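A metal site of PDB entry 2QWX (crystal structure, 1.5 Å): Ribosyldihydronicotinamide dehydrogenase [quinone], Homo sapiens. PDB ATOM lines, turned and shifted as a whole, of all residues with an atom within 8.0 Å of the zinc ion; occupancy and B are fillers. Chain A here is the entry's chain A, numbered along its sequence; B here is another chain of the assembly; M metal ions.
A ring nitrogen (NE2) of His 174 sits close to the side-chain hydroxyl (OH) of Tyr 133.
O of His 174 is in hydrogen-bond range of N of Phe 179 (3.1 Å).
O of Val 161 of chain B lies within hydrogen-bond range of NE2 of His 174, at 3.1 Å.
The side-chain sulfur of Cys 223 sits close to the backbone carbonyl oxygen of Gln 173.
The backbone carbonyl oxygen (O) of Gln 173 lies within hydrogen-bond range of the backbone NH (N) of His 178.
The side-chain carboxylate of Asp 134 lies within hydrogen-bond range of a ring nitrogen (NE2) of His 178 (2.9 Å).
Three residues have an atom within 4 Å of the zinc ion: His 174, His 178 and Cys 223.
ND1 of His 174 is bound to the zinc ion (2.1 Å).
O of Cys 223 binds the zinc ion (2.1 Å).
The zinc ion is bound by a ring nitrogen (ND1) of His 178 (2.1 Å).
SG of Cys 223 is bound to the zinc ion.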
ATOM      1  N   TYR A 133      -4.410  15.108  30.441  1.00  0.00           N
ATOM      2  CA  TYR A 133      -4.281  16.526  30.151  1.00  0.00           C
ATOM      3  C   TYR A 133      -2.843  16.769  29.665  1.00  0.00           C
ATOM      4  O   TYR A 133      -2.402  16.108  28.725  1.00  0.00           O
ATOM      5  CB  TYR A 133      -4.692  17.422  31.335  1.00  0.00           C
ATOM      6  CG  TYR A 133      -6.212  17.505  31.438  1.00  0.00           C
ATOM      7  CD1 TYR A 133      -6.995  17.798  30.323  1.00  0.00           C
ATOM      8  CD2 TYR A 133      -6.862  17.197  32.626  1.00  0.00           C
ATOM      9  CE1 TYR A 133      -8.409  17.767  30.381  1.00  0.00           C
ATOM     10  CE2 TYR A 133      -8.265  17.173  32.701  1.00  0.00           C
ATOM     11  CZ  TYR A 133      -9.024  17.449  31.579  1.00  0.00           C
ATOM     12  OH  TYR A 133     -10.408  17.378  31.698  1.00  0.00           O
ATOM     13  N   ASP A 134      -2.095  17.698  30.252  1.00  0.00           N
ATOM     14  CA  ASP A 134      -0.773  17.927  29.727  1.00  0.00           C
ATOM     15  C   ASP A 134       0.128  16.704  29.767  1.00  0.00           C
ATOM     16  O   ASP A 134       1.110  16.665  29.033  1.00  0.00           O
ATOM     17  CB  ASP A 134      -0.104  19.107  30.416  1.00  0.00           C
ATOM     18  CG  ASP A 134      -0.715  20.449  30.021  1.00  0.00           C
ATOM     19  OD1 ASP A 134      -1.519  20.528  29.066  1.00  0.00           O
ATOM     20  OD2 ASP A 134      -0.367  21.464  30.676  1.00  0.00           O
ATOM     21  N   TRP A 170     -16.201  22.355  24.083  1.00  0.00           N
ATOM     22  CA  TRP A 170     -15.526  21.942  25.306  1.00  0.00           C
ATOM     23  C   TRP A 170     -15.319  20.444  25.579  1.00  0.00           C
ATOM     24  O   TRP A 170     -14.213  20.012  25.852  1.00  0.00           O
ATOM     25  CB  TRP A 170     -16.240  22.613  26.512  1.00  0.00           C
ATOM     26  CG  TRP A 170     -15.743  22.243  27.866  1.00  0.00           C
ATOM     27  CD1 TRP A 170     -16.419  21.470  28.782  1.00  0.00           C
ATOM     28  CD2 TRP A 170     -14.577  22.725  28.537  1.00  0.00           C
ATOM     29  NE1 TRP A 170     -15.750  21.461  29.965  1.00  0.00           N
ATOM     30  CE2 TRP A 170     -14.618  22.232  29.852  1.00  0.00           C
ATOM     31  CE3 TRP A 170     -13.512  23.549  28.150  1.00  0.00           C
ATOM     32  CZ2 TRP A 170     -13.635  22.527  30.798  1.00  0.00           C
ATOM     33  CZ3 TRP A 170     -12.521  23.846  29.090  1.00  0.00           C
ATOM     34  CH2 TRP A 170     -12.596  23.330  30.404  1.00  0.00           C
ATOM     35  N   LEU A 172     -15.250  18.047  23.555  1.00  0.00           N
ATOM     36  CA  LEU A 172     -14.390  17.499  22.529  1.00  0.00           C
ATOM     37  C   LEU A 172     -12.962  17.980  22.586  1.00  0.00           C
ATOM     38  O   LEU A 172     -12.045  17.176  22.686  1.00  0.00           O
ATOM     39  CB  LEU A 172     -14.987  17.815  21.145  1.00  0.00           C
ATOM     40  CG  LEU A 172     -16.417  17.304  20.907  1.00  0.00           C
ATOM     41  CD1 LEU A 172     -16.992  17.904  19.601  1.00  0.00           C
ATOM     42  CD2 LEU A 172     -16.380  15.774  20.877  1.00  0.00           C
ATOM     43  N   GLN A 173     -12.765  19.294  22.576  1.00  0.00           N
ATOM     44  CA  GLN A 173     -11.407  19.793  22.614  1.00  0.00           C
ATOM     45  C   GLN A 173     -10.737  19.575  23.939  1.00  0.00           C
ATOM     46  O   GLN A 173      -9.587  19.157  23.988  1.00  0.00           O
ATOM     47  CB  GLN A 173     -11.360  21.288  22.256  1.00  0.00           C
ATOM     48  CG  GLN A 173     -11.830  21.524  20.814  1.00  0.00           C
ATOM     49  CD  GLN A 173     -11.614  22.948  20.305  1.00  0.00           C
ATOM     50  OE1 GLN A 173     -11.417  23.166  19.117  1.00  0.00           O
ATOM     51  NE2 GLN A 173     -11.679  23.933  21.215  1.00  0.00           N
ATOM     52  N   HIS A 174     -11.446  19.893  25.013  1.00  0.00           N
ATOM     53  CA  HIS A 174     -10.857  19.753  26.320  1.00  0.00           C
ATOM     54  C   HIS A 174     -11.016  18.402  26.959  1.00  0.00           C
ATOM     55  O   HIS A 174     -10.023  17.753  27.373  1.00  0.00           O
ATOM     56  CB  HIS A 174     -11.439  20.829  27.263  1.00  0.00           C
ATOM     57  CG  HIS A 174     -10.777  20.844  28.595  1.00  0.00           C
ATOM     58  ND1 HIS A 174      -9.541  21.403  28.810  1.00  0.00           N
ATOM     59  CD2 HIS A 174     -11.179  20.343  29.784  1.00  0.00           C
ATOM     60  CE1 HIS A 174      -9.209  21.248  30.076  1.00  0.00           C
ATOM     61  NE2 HIS A 174     -10.182  20.605  30.689  1.00  0.00           N
ATOM     62  N   GLY A 175     -12.258  17.963  27.042  1.00  0.00           N
ATOM     63  CA  GLY A 175     -12.574  16.733  27.727  1.00  0.00           C
ATOM     64  C   GLY A 175     -12.026  15.493  27.061  1.00  0.00           C
ATOM     65  O   GLY A 175     -11.760  14.478  27.736  1.00  0.00           O
ATOM     66  N   THR A 176     -11.769  15.583  25.762  1.00  0.00           N
ATOM     67  CA  THR A 176     -11.284  14.429  25.039  1.00  0.00           C
ATOM     68  C   THR A 176      -9.885  14.638  24.490  1.00  0.00           C
ATOM     69  O   THR A 176      -8.951  13.946  24.882  1.00  0.00           O
ATOM     70  CB  THR A 176     -12.251  14.087  23.847  1.00  0.00           C
ATOM     71  OG1 THR A 176     -13.598  13.974  24.340  1.00  0.00           O
ATOM     72  CG2 THR A 176     -11.853  12.743  23.171  1.00  0.00           C
ATOM     73  N   LEU A 177      -9.715  15.599  23.584  1.00  0.00           N
ATOM     74  CA  LEU A 177      -8.403  15.776  22.946  1.00  0.00           C
ATOM     75  C   LEU A 177      -7.311  16.242  23.901  1.00  0.00           C
ATOM     76  O   LEU A 177      -6.271  15.587  24.023  1.00  0.00           O
ATOM     77  CB  LEU A 177      -8.560  16.692  21.729  1.00  0.00           C
ATOM     78  CG  LEU A 177      -9.557  16.182  20.669  1.00  0.00           C
ATOM     79  CD1 LEU A 177      -9.727  17.257  19.582  1.00  0.00           C
ATOM     80  CD2 LEU A 177      -9.077  14.830  20.082  1.00  0.00           C
ATOM     81  N   HIS A 178      -7.556  17.336  24.621  1.00  0.00           N
ATOM     82  CA  HIS A 178      -6.532  17.790  25.551  1.00  0.00           C
ATOM     83  C   HIS A 178      -6.350  16.723  26.655  1.00  0.00           C
ATOM     84  O   HIS A 178      -5.221  16.468  27.095  1.00  0.00           O
ATOM     85  CB  HIS A 178      -7.018  19.121  26.141  1.00  0.00           C
ATOM     86  CG  HIS A 178      -6.048  19.786  27.061  1.00  0.00           C
ATOM     87  ND1 HIS A 178      -6.322  20.976  27.686  1.00  0.00           N
ATOM     88  CD2 HIS A 178      -4.791  19.441  27.441  1.00  0.00           C
ATOM     89  CE1 HIS A 178      -5.279  21.346  28.414  1.00  0.00           C
ATOM     90  NE2 HIS A 178      -4.346  20.431  28.285  1.00  0.00           N
ATOM     91  N   PHE A 179      -7.433  16.072  27.087  1.00  0.00           N
ATOM     92  CA  PHE A 179      -7.303  15.063  28.124  1.00  0.00           C
ATOM     93  C   PHE A 179      -6.285  13.993  27.707  1.00  0.00           C
ATOM     94  O   PHE A 179      -5.528  13.451  28.547  1.00  0.00           O
ATOM     95  CB  PHE A 179      -8.675  14.411  28.425  1.00  0.00           C
ATOM     96  CG  PHE A 179      -8.658  13.463  29.582  1.00  0.00           C
ATOM     97  CD1 PHE A 179      -8.870  13.939  30.871  1.00  0.00           C
ATOM     98  CD2 PHE A 179      -8.432  12.098  29.396  1.00  0.00           C
ATOM     99  CE1 PHE A 179      -8.862  13.042  31.964  1.00  0.00           C
ATOM    100  CE2 PHE A 179      -8.415  11.215  30.471  1.00  0.00           C
ATOM    101  CZ  PHE A 179      -8.635  11.680  31.764  1.00  0.00           C
ATOM    102  N   PHE A 182      -3.222  15.727  23.412  1.00  0.00           N
ATOM    103  CA  PHE A 182      -3.082  16.477  22.186  1.00  0.00           C
ATOM    104  C   PHE A 182      -3.001  17.993  22.417  1.00  0.00           C
ATOM    105  O   PHE A 182      -3.561  18.524  23.397  1.00  0.00           O
ATOM    106  CB  PHE A 182      -4.330  16.347  21.275  1.00  0.00           C
ATOM    107  CG  PHE A 182      -4.482  15.029  20.587  1.00  0.00           C
ATOM    108  CD1 PHE A 182      -3.797  14.757  19.410  1.00  0.00           C
ATOM    109  CD2 PHE A 182      -5.418  14.098  21.064  1.00  0.00           C
ATOM    110  CE1 PHE A 182      -4.031  13.584  18.725  1.00  0.00           C
ATOM    111  CE2 PHE A 182      -5.663  12.904  20.374  1.00  0.00           C
ATOM    112  CZ  PHE A 182      -4.950  12.669  19.178  1.00  0.00           C
ATOM    113  N   VAL A 184      -4.310  21.210  20.709  1.00  0.00           N
ATOM    114  CA  VAL A 184      -5.436  21.461  19.834  1.00  0.00           C
ATOM    115  C   VAL A 184      -5.298  22.695  18.982  1.00  0.00           C
ATOM    116  O   VAL A 184      -5.096  23.802  19.505  1.00  0.00           O
ATOM    117  CB  VAL A 184      -6.721  21.580  20.712  1.00  0.00           C
ATOM    118  CG1 VAL A 184      -7.961  21.812  19.833  1.00  0.00           C
ATOM    119  CG2 VAL A 184      -6.865  20.315  21.564  1.00  0.00           C
ATOM    120  N   ILE A 221      -4.333  26.307  20.355  1.00  0.00           N
ATOM    121  CA  ILE A 221      -5.056  27.247  21.189  1.00  0.00           C
ATOM    122  C   ILE A 221      -4.762  26.932  22.645  1.00  0.00           C
ATOM    123  O   ILE A 221      -4.248  25.878  22.981  1.00  0.00           O
ATOM    124  CB  ILE A 221      -6.581  27.095  21.066  1.00  0.00           C
ATOM    125  CG1 ILE A 221      -6.984  25.706  21.573  1.00  0.00           C
ATOM    126  CG2 ILE A 221      -7.018  27.397  19.670  1.00  0.00           C
ATOM    127  CD1 ILE A 221      -8.477  25.522  21.701  1.00  0.00           C
ATOM    128  N   PRO A 222      -5.016  27.904  23.536  1.00  0.00           N
ATOM    129  CA  PRO A 222      -4.773  27.593  24.943  1.00  0.00           C
ATOM    130  C   PRO A 222      -6.122  26.925  25.288  1.00  0.00           C
ATOM    131  O   PRO A 222      -7.150  27.592  25.388  1.00  0.00           O
ATOM    132  CB  PRO A 222      -4.561  28.987  25.580  1.00  0.00           C
ATOM    133  CG  PRO A 222      -5.361  29.904  24.675  1.00  0.00           C
ATOM    134  CD  PRO A 222      -5.095  29.358  23.286  1.00  0.00           C
ATOM    135  N   CYS A 223      -6.129  25.603  25.378  1.00  0.00           N
ATOM    136  CA  CYS A 223      -7.358  24.842  25.619  1.00  0.00           C
ATOM    137  C   CYS A 223      -7.754  24.904  27.082  1.00  0.00           C
ATOM    138  O   CYS A 223      -7.582  23.937  27.849  1.00  0.00           O
ATOM    139  CB  CYS A 223      -7.139  23.383  25.161  1.00  0.00           C
ATOM    140  SG  CYS A 223      -8.607  22.377  25.166  1.00  0.00           S
ATOM    141  N   THR A 224      -8.293  26.053  27.464  1.00  0.00           N
ATOM    142  CA  THR A 224      -8.660  26.295  28.849  1.00  0.00           C
ATOM    143  C   THR A 224     -10.107  26.702  28.942  1.00  0.00           C
ATOM    144  O   THR A 224     -10.759  26.957  27.938  1.00  0.00           O
ATOM    145  CB  THR A 224      -7.803  27.438  29.374  1.00  0.00           C
ATOM    146  OG1 THR A 224      -8.097  28.593  28.583  1.00  0.00           O
ATOM    147  CG2 THR A 224      -6.346  27.136  29.207  1.00  0.00           C
ATOM    148  N   ALA A 225     -10.617  26.785  30.177  1.00  0.00           N
ATOM    149  CA  ALA A 225     -11.982  27.252  30.379  1.00  0.00           C
ATOM    150  C   ALA A 225     -12.094  28.703  29.899  1.00  0.00           C
ATOM    151  O   ALA A 225     -13.073  29.093  29.293  1.00  0.00           O
ATOM    152  CB  ALA A 225     -12.370  27.159  31.857  1.00  0.00           C
ATOM    153  N   TRP A 227     -10.585  30.229  27.395  1.00  0.00           N
ATOM    154  CA  TRP A 227     -10.697  30.285  25.934  1.00  0.00           C
ATOM    155  C   TRP A 227     -12.111  29.899  25.520  1.00  0.00           C
ATOM    156  O   TRP A 227     -12.723  30.502  24.637  1.00  0.00           O
ATOM    157  CB  TRP A 227      -9.690  29.304  25.294  1.00  0.00           C
ATOM    158  CG  TRP A 227      -9.646  29.374  23.776  1.00  0.00           C
ATOM    159  CD1 TRP A 227      -8.846  30.209  23.025  1.00  0.00           C
ATOM    160  CD2 TRP A 227     -10.457  28.636  22.826  1.00  0.00           C
ATOM    161  NE1 TRP A 227      -9.110  30.037  21.684  1.00  0.00           N
ATOM    162  CE2 TRP A 227     -10.096  29.091  21.536  1.00  0.00           C
ATOM    163  CE3 TRP A 227     -11.463  27.660  22.945  1.00  0.00           C
ATOM    164  CZ2 TRP A 227     -10.686  28.593  20.376  1.00  0.00           C
ATOM    165  CZ3 TRP A 227     -12.046  27.174  21.781  1.00  0.00           C
ATOM    166  CH2 TRP A 227     -11.653  27.637  20.518  1.00  0.00           C
ATOM    167  N   HIS A 228     -12.638  28.854  26.149  1.00  0.00           N
ATOM    168  CA  HIS A 228     -13.968  28.384  25.787  1.00  0.00           C
ATOM    169  C   HIS A 228     -15.165  29.192  26.276  1.00  0.00           C
ATOM    170  O   HIS A 228     -16.134  29.371  25.538  1.00  0.00           O
ATOM    171  CB  HIS A 228     -14.162  26.927  26.263  1.00  0.00           C
ATOM    172  CG  HIS A 228     -13.381  25.903  25.464  1.00  0.00           C
ATOM    173  ND1 HIS A 228     -12.079  25.565  25.772  1.00  0.00           N
ATOM    174  CD2 HIS A 228     -13.732  25.133  24.406  1.00  0.00           C
ATOM    175  CE1 HIS A 228     -11.655  24.630  24.930  1.00  0.00           C
ATOM    176  NE2 HIS A 228     -12.646  24.346  24.094  1.00  0.00           N
ATOM    177  N   VAL B 161      -9.595  20.409  37.358  1.00  0.00           N
ATOM    178  CA  VAL B 161      -9.065  20.057  36.038  1.00  0.00           C
ATOM    179  C   VAL B 161     -10.104  19.846  34.942  1.00  0.00           C
ATOM    180  O   VAL B 161      -9.865  20.167  33.770  1.00  0.00           O
ATOM    181  CB  VAL B 161      -8.157  18.811  36.097  1.00  0.00           C
ATOM    182  CG1 VAL B 161      -6.869  19.152  36.821  1.00  0.00           C
ATOM    183  CG2 VAL B 161      -8.881  17.653  36.753  1.00  0.00           C
HETATM  184 ZN    ZN M   1      -8.165  21.984  27.365  1.00  0.00          ZN
